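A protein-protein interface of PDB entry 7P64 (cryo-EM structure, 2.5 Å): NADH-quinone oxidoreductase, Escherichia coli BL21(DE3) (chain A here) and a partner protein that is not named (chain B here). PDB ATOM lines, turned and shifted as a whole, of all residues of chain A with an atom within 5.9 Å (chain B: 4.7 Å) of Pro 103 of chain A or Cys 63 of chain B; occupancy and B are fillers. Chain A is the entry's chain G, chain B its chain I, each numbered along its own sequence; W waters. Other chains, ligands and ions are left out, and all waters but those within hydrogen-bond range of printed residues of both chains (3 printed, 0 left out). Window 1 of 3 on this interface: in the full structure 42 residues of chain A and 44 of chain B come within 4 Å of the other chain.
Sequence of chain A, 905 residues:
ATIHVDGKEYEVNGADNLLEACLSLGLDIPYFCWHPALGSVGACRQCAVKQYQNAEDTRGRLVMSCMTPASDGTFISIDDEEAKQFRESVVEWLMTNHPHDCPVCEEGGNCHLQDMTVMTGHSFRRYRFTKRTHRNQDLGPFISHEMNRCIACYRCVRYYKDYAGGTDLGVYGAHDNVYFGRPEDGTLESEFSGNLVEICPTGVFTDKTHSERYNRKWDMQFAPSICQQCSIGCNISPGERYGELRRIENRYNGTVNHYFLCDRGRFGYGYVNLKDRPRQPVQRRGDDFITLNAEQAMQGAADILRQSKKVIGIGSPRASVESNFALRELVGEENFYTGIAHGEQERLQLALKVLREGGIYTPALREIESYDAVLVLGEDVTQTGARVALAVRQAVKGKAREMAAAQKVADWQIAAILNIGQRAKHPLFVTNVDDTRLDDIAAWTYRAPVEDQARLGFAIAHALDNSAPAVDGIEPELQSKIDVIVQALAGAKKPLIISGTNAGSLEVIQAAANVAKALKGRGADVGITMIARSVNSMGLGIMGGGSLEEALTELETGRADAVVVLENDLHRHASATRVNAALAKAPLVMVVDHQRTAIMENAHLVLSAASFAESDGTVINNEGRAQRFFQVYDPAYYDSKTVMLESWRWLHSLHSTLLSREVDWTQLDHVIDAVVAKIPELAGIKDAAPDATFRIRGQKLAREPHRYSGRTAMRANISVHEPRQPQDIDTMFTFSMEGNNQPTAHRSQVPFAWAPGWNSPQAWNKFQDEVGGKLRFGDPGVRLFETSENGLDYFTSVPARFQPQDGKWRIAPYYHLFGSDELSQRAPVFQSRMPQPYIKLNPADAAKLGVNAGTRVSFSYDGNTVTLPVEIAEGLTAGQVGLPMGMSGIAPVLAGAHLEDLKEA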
ATOM      1  N   HIS A 100       9.659  27.570 -17.317  1.00  0.00           N
ATOM      2  CA  HIS A 100      10.105  27.808 -18.689  1.00  0.00           C
ATOM      3  C   HIS A 100      11.053  26.692 -19.141  1.00  0.00           C
ATOM      4  O   HIS A 100      12.232  26.904 -19.410  1.00  0.00           O
ATOM      5  CB  HIS A 100      10.774  29.174 -18.758  1.00  0.00           C
ATOM      6  CG  HIS A 100      10.956  29.706 -20.145  1.00  0.00           C
ATOM      7  ND1 HIS A 100      10.003  30.469 -20.780  1.00  0.00           N
ATOM      8  CD2 HIS A 100      11.995  29.609 -21.006  1.00  0.00           C
ATOM      9  CE1 HIS A 100      10.439  30.805 -21.980  1.00  0.00           C
ATOM     10  NE2 HIS A 100      11.646  30.296 -22.142  1.00  0.00           N
ATOM     11  N   ASP A 101      10.511  25.478 -19.236  1.00  0.00           N
ATOM     12  CA  ASP A 101      11.338  24.283 -19.196  1.00  0.00           C
ATOM     13  C   ASP A 101      11.284  23.389 -20.425  1.00  0.00           C
ATOM     14  O   ASP A 101      12.059  22.432 -20.472  1.00  0.00           O
ATOM     15  CB  ASP A 101      10.966  23.423 -17.979  1.00  0.00           C
ATOM     16  CG  ASP A 101      11.869  23.655 -16.800  1.00  0.00           C
ATOM     17  OD1 ASP A 101      12.615  24.649 -16.805  1.00  0.00           O
ATOM     18  OD2 ASP A 101      11.832  22.830 -15.867  1.00  0.00           O
ATOM     19  N   CYS A 102      10.417  23.663 -21.403  1.00  0.00           N
ATOM     20  CA  CYS A 102      10.217  22.758 -22.539  1.00  0.00           C
ATOM     21  C   CYS A 102      11.483  22.342 -23.298  1.00  0.00           C
ATOM     22  O   CYS A 102      11.558  21.165 -23.686  1.00  0.00           O
ATOM     23  CB  CYS A 102       9.217  23.363 -23.538  1.00  0.00           C
ATOM     24  SG  CYS A 102       7.551  23.654 -22.959  1.00  0.00           S
ATOM     25  N   PRO A 103      12.474  23.211 -23.570  1.00  0.00           N
ATOM     26  CA  PRO A 103      13.702  22.706 -24.213  1.00  0.00           C
ATOM     27  C   PRO A 103      14.475  21.682 -23.396  1.00  0.00           C
ATOM     28  O   PRO A 103      15.113  20.803 -23.982  1.00  0.00           O
ATOM     29  CB  PRO A 103      14.526  23.981 -24.431  1.00  0.00           C
ATOM     30  CG  PRO A 103      13.545  25.037 -24.503  1.00  0.00           C
ATOM     31  CD  PRO A 103      12.502  24.685 -23.518  1.00  0.00           C
ATOM     32  N   VAL A 104      14.433  21.753 -22.070  1.00  0.00           N
ATOM     33  CA  VAL A 104      15.223  20.850 -21.240  1.00  0.00           C
ATOM     34  C   VAL A 104      14.309  19.905 -20.477  1.00  0.00           C
ATOM     35  O   VAL A 104      14.650  19.438 -19.386  1.00  0.00           O
ATOM     36  CB  VAL A 104      16.125  21.636 -20.273  1.00  0.00           C
ATOM     37  CG1 VAL A 104      17.276  22.242 -21.026  1.00  0.00           C
ATOM     38  CG2 VAL A 104      15.328  22.709 -19.558  1.00  0.00           C
ATOM     39  N   CYS A 105      13.147  19.617 -21.040  1.00  0.00           N
ATOM     40  CA  CYS A 105      12.171  18.741 -20.417  1.00  0.00           C
ATOM     41  C   CYS A 105      11.977  17.522 -21.300  1.00  0.00           C
ATOM     42  O   CYS A 105      11.743  17.656 -22.504  1.00  0.00           O
ATOM     43  CB  CYS A 105      10.852  19.472 -20.204  1.00  0.00           C
ATOM     44  SG  CYS A 105       9.509  18.519 -19.517  1.00  0.00           S
ATOM     45  N   ARG A 216      13.881  13.059 -28.772  1.00  0.00           N
ATOM     46  CA  ARG A 216      12.475  13.423 -28.831  1.00  0.00           C
ATOM     47  C   ARG A 216      11.662  12.340 -29.536  1.00  0.00           C
ATOM     48  O   ARG A 216      12.199  11.462 -30.212  1.00  0.00           O
ATOM     49  CB  ARG A 216      12.310  14.766 -29.529  1.00  0.00           C
ATOM     50  CG  ARG A 216      13.095  15.876 -28.876  1.00  0.00           C
ATOM     51  CD  ARG A 216      12.285  16.546 -27.796  1.00  0.00           C
ATOM     52  NE  ARG A 216      12.986  17.683 -27.219  1.00  0.00           N
ATOM     53  CZ  ARG A 216      12.827  18.103 -25.973  1.00  0.00           C
ATOM     54  NH1 ARG A 216      11.995  17.501 -25.145  1.00  0.00           N
ATOM     55  NH2 ARG A 216      13.526  19.148 -25.547  1.00  0.00           N
ATOM     56  N   TRP A 218       9.544  12.517 -32.050  1.00  0.00           N
ATOM     57  CA  TRP A 218       9.553  12.560 -33.508  1.00  0.00           C
ATOM     58  C   TRP A 218      10.819  11.957 -34.105  1.00  0.00           C
ATOM     59  O   TRP A 218      10.814  11.586 -35.280  1.00  0.00           O
ATOM     60  CB  TRP A 218       9.378  13.997 -33.999  1.00  0.00           C
ATOM     61  CG  TRP A 218      10.407  14.970 -33.497  1.00  0.00           C
ATOM     62  CD1 TRP A 218      11.695  15.092 -33.918  1.00  0.00           C
ATOM     63  CD2 TRP A 218      10.221  15.972 -32.492  1.00  0.00           C
ATOM     64  NE1 TRP A 218      12.327  16.089 -33.229  1.00  0.00           N
ATOM     65  CE2 TRP A 218      11.441  16.654 -32.354  1.00  0.00           C
ATOM     66  CE3 TRP A 218       9.143  16.353 -31.694  1.00  0.00           C
ATOM     67  CZ2 TRP A 218      11.612  17.699 -31.454  1.00  0.00           C
ATOM     68  CZ3 TRP A 218       9.317  17.384 -30.798  1.00  0.00           C
ATOM     69  CH2 TRP A 218      10.542  18.044 -30.685  1.00  0.00           C
ATOM     70  N   VAL B  61      21.185  23.643 -25.501  1.00  0.00           N
ATOM     71  CA  VAL B  61      20.699  22.704 -24.506  1.00  0.00           C
ATOM     72  C   VAL B  61      20.280  21.387 -25.140  1.00  0.00           C
ATOM     73  O   VAL B  61      19.624  20.575 -24.489  1.00  0.00           O
ATOM     74  CB  VAL B  61      19.550  23.318 -23.694  1.00  0.00           C
ATOM     75  CG1 VAL B  61      20.002  24.605 -23.054  1.00  0.00           C
ATOM     76  CG2 VAL B  61      18.340  23.562 -24.572  1.00  0.00           C
ATOM     77  N   ALA B  62      20.636  21.171 -26.410  1.00  0.00           N
ATOM     78  CA  ALA B  62      20.373  19.933 -27.142  1.00  0.00           C
ATOM     79  C   ALA B  62      18.889  19.575 -27.144  1.00  0.00           C
ATOM     80  O   ALA B  62      18.505  18.419 -26.976  1.00  0.00           O
ATOM     81  CB  ALA B  62      21.216  18.783 -26.602  1.00  0.00           C
ATOM     82  N   CYS B  63      18.051  20.585 -27.327  1.00  0.00           N
ATOM     83  CA  CYS B  63      16.611  20.407 -27.310  1.00  0.00           C
ATOM     84  C   CYS B  63      16.061  19.839 -28.612  1.00  0.00           C
ATOM     85  O   CYS B  63      14.883  19.472 -28.649  1.00  0.00           O
ATOM     86  CB  CYS B  63      15.945  21.742 -27.000  1.00  0.00           C
ATOM     87  SG  CYS B  63      15.760  22.818 -28.399  1.00  0.00           S
ATOM     88  N   ASN B  64      16.880  19.784 -29.666  1.00  0.00           N
ATOM     89  CA  ASN B  64      16.579  19.177 -30.962  1.00  0.00           C
ATOM     90  C   ASN B  64      15.474  19.889 -31.732  1.00  0.00           C
ATOM     91  O   ASN B  64      14.880  19.298 -32.633  1.00  0.00           O
ATOM     92  CB  ASN B  64      16.232  17.687 -30.825  1.00  0.00           C
ATOM     93  CG  ASN B  64      17.383  16.787 -31.191  1.00  0.00           C
ATOM     94  OD1 ASN B  64      17.712  16.629 -32.362  1.00  0.00           O
ATOM     95  ND2 ASN B  64      18.007  16.193 -30.189  1.00  0.00           N
ATOM     96  N   LEU B  65      15.184  21.153 -31.424  1.00  0.00           N
ATOM     97  CA  LEU B  65      14.176  21.872 -32.197  1.00  0.00           C
ATOM     98  C   LEU B  65      14.708  22.296 -33.561  1.00  0.00           C
ATOM     99  O   LEU B  65      13.964  22.300 -34.547  1.00  0.00           O
ATOM    100  CB  LEU B  65      13.676  23.089 -31.420  1.00  0.00           C
ATOM    101  CG  LEU B  65      12.615  22.862 -30.339  1.00  0.00           C
ATOM    102  CD1 LEU B  65      12.027  24.186 -29.894  1.00  0.00           C
ATOM    103  CD2 LEU B  65      11.522  21.916 -30.802  1.00  0.00           C
ATOM    104  N   TRP B  87      21.736  20.554 -19.649  1.00  0.00           N
ATOM    105  CA  TRP B  87      21.743  19.842 -20.913  1.00  0.00           C
ATOM    106  C   TRP B  87      22.709  20.515 -21.877  1.00  0.00           C
ATOM    107  O   TRP B  87      22.860  21.739 -21.881  1.00  0.00           O
ATOM    108  CB  TRP B  87      20.347  19.823 -21.522  1.00  0.00           C
ATOM    109  CG  TRP B  87      19.324  18.972 -20.842  1.00  0.00           C
ATOM    110  CD1 TRP B  87      19.296  18.592 -19.535  1.00  0.00           C
ATOM    111  CD2 TRP B  87      18.158  18.411 -21.446  1.00  0.00           C
ATOM    112  NE1 TRP B  87      18.192  17.822 -19.291  1.00  0.00           N
ATOM    113  CE2 TRP B  87      17.475  17.696 -20.449  1.00  0.00           C
ATOM    114  CE3 TRP B  87      17.629  18.439 -22.739  1.00  0.00           C
ATOM    115  CZ2 TRP B  87      16.293  17.013 -20.704  1.00  0.00           C
ATOM    116  CZ3 TRP B  87      16.457  17.766 -22.988  1.00  0.00           C
ATOM    117  CH2 TRP B  87      15.800  17.061 -21.976  1.00  0.00           C
ATOM    118  N   PRO B 110      15.183  28.023 -29.215  1.00  0.00           N
ATOM    119  CA  PRO B 110      14.655  28.742 -28.056  1.00  0.00           C
ATOM    120  C   PRO B 110      15.720  29.287 -27.119  1.00  0.00           C
ATOM    121  O   PRO B 110      15.370  29.903 -26.110  1.00  0.00           O
ATOM    122  CB  PRO B 110      13.816  27.667 -27.361  1.00  0.00           C
ATOM    123  CG  PRO B 110      14.524  26.405 -27.680  1.00  0.00           C
ATOM    124  CD  PRO B 110      15.185  26.566 -29.011  1.00  0.00           C
ATOM    125  N   PHE B 150      19.165  31.255 -21.662  1.00  0.00           N
ATOM    126  CA  PHE B 150      17.996  30.419 -21.413  1.00  0.00           C
ATOM    127  C   PHE B 150      17.967  29.907 -19.983  1.00  0.00           C
ATOM    128  O   PHE B 150      16.893  29.781 -19.390  1.00  0.00           O
ATOM    129  CB  PHE B 150      17.976  29.252 -22.401  1.00  0.00           C
ATOM    130  CG  PHE B 150      16.996  28.170 -22.052  1.00  0.00           C
ATOM    131  CD1 PHE B 150      15.644  28.343 -22.286  1.00  0.00           C
ATOM    132  CD2 PHE B 150      17.429  26.974 -21.499  1.00  0.00           C
ATOM    133  CE1 PHE B 150      14.744  27.353 -21.971  1.00  0.00           C
ATOM    134  CE2 PHE B 150      16.532  25.983 -21.180  1.00  0.00           C
ATOM    135  CZ  PHE B 150      15.186  26.172 -21.417  1.00  0.00           C
HETATM  136  O   HOH W   1      15.748  14.077 -30.756  1.00  0.00           O
HETATM  137  O   HOH W   2      13.164  30.223 -24.330  1.00  0.00           O
HETATM  138  O   HOH W   3      14.865  16.655 -33.803  1.00  0.00           O
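O of Cys 102 of chain A lies within hydrogen-bond range of NH2 of Arg 216 of chain A, 3.4 Å away. The backbone carbonyl oxygen of Pro 103 of chain A lies within hydrogen-bond range of the guanidinium group of Arg 216 of chain A (2.8 Å). O of Cys 105 of chain A sits at hydrogen-bond distance from NH1 of Arg 216 of chain A. The side-chain sulfur (SG) of Cys 63 of chain B lies close to the backbone NH (N) of Leu 65 of chain B (3.5 Å).
Printed residues of chain B that touch a printed residue of chain A: Val 61, Cys 63, Asn 64, Leu 65, Trp 87, Pro 110 and Phe 150. Of the 8 printed residues of chain A, 6 touch a printed residue of chain B. Hydrophobic or aromatic side chains of chain A that line the printed part of chain B: His 100, Pro 103, Val 104 and Trp 218.
The guanidinium group (NE) of Arg 216 of chain A sits at hydrogen-bond distance from the backbone carbonyl oxygen (O) of Cys 63 of chain B (3.0 Å).
Water W3 bridges the indole nitrogen (NE1) of Trp 218 of chain A and the backbone carbonyl oxygen (O) of Asn 64 of chain B. Water W2 bridges NE2 of His 100 of chain A (2.7 Å) and O of Pro 110 of chain B (2.9 Å). Water W1 lies within hydrogen-bond range of N of Arg 216 of chain A (2.9 Å) and ND2 of Asn 64 of chain B (3.1 Å).
Pro 103 of chain A touches just these residues of chain B: Val 61, Cys 63, Trp 87, Pro 110 and Phe 150. Of chain A, only Pro 103 (3.3 Å) and Arg 216 (3.0 Å) come within 4 Å of Cys 63 of chain B. Printed residues of chain B within 4 Å of Cys 105 of chain A: Trp 87. Of the printed residues of chain B, Arg 216 of chain A touches Cys 63 (3.0 Å). Of the printed residues of chain B, His 100 of chain A touches Phe 150 (3.6 Å). Of the printed residues of chain B, Val 104 of chain A touches Val 61 (3.7 Å), Trp 87 (3.2 Å) and Phe 150 (3.8 Å). Of the printed residues of chain B, Trp 218 of chain A touches Asn 64 and Leu 65. Cys 102 of chain A touches none of the printed residues of chain B.
Among the printed residues, merely in contact across the chains: His 100 of chain A with Phe 150 of chain B (3.6 Å), Pro 103 of chain A with Val 61 of chain B (3.8 Å), Pro 103 of chain A with Cys 63 of chain B (3.3 Å), Pro 103 of chain A with Trp 87 of chain B (3.5 Å), Pro 103 of chain A with Pro 110 of chain B (3.6 Å), Pro 103 of chain A with Phe 150 of chain B (3.6 Å), Val 104 of chain A with Val 61 of chain B (3.7 Å), Val 104 of chain A with Trp 87 of chain B (3.2 Å), Val 104 of chain A with Phe 150 of chain B (3.8 Å), Cys 105 of chain A with Trp 87 of chain B (3.8 Å), Trp 218 of chain A with Asn 64 of chain B (3.8 Å) and Trp 218 of chain A with Leu 65 of chain B (3.996 Å).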
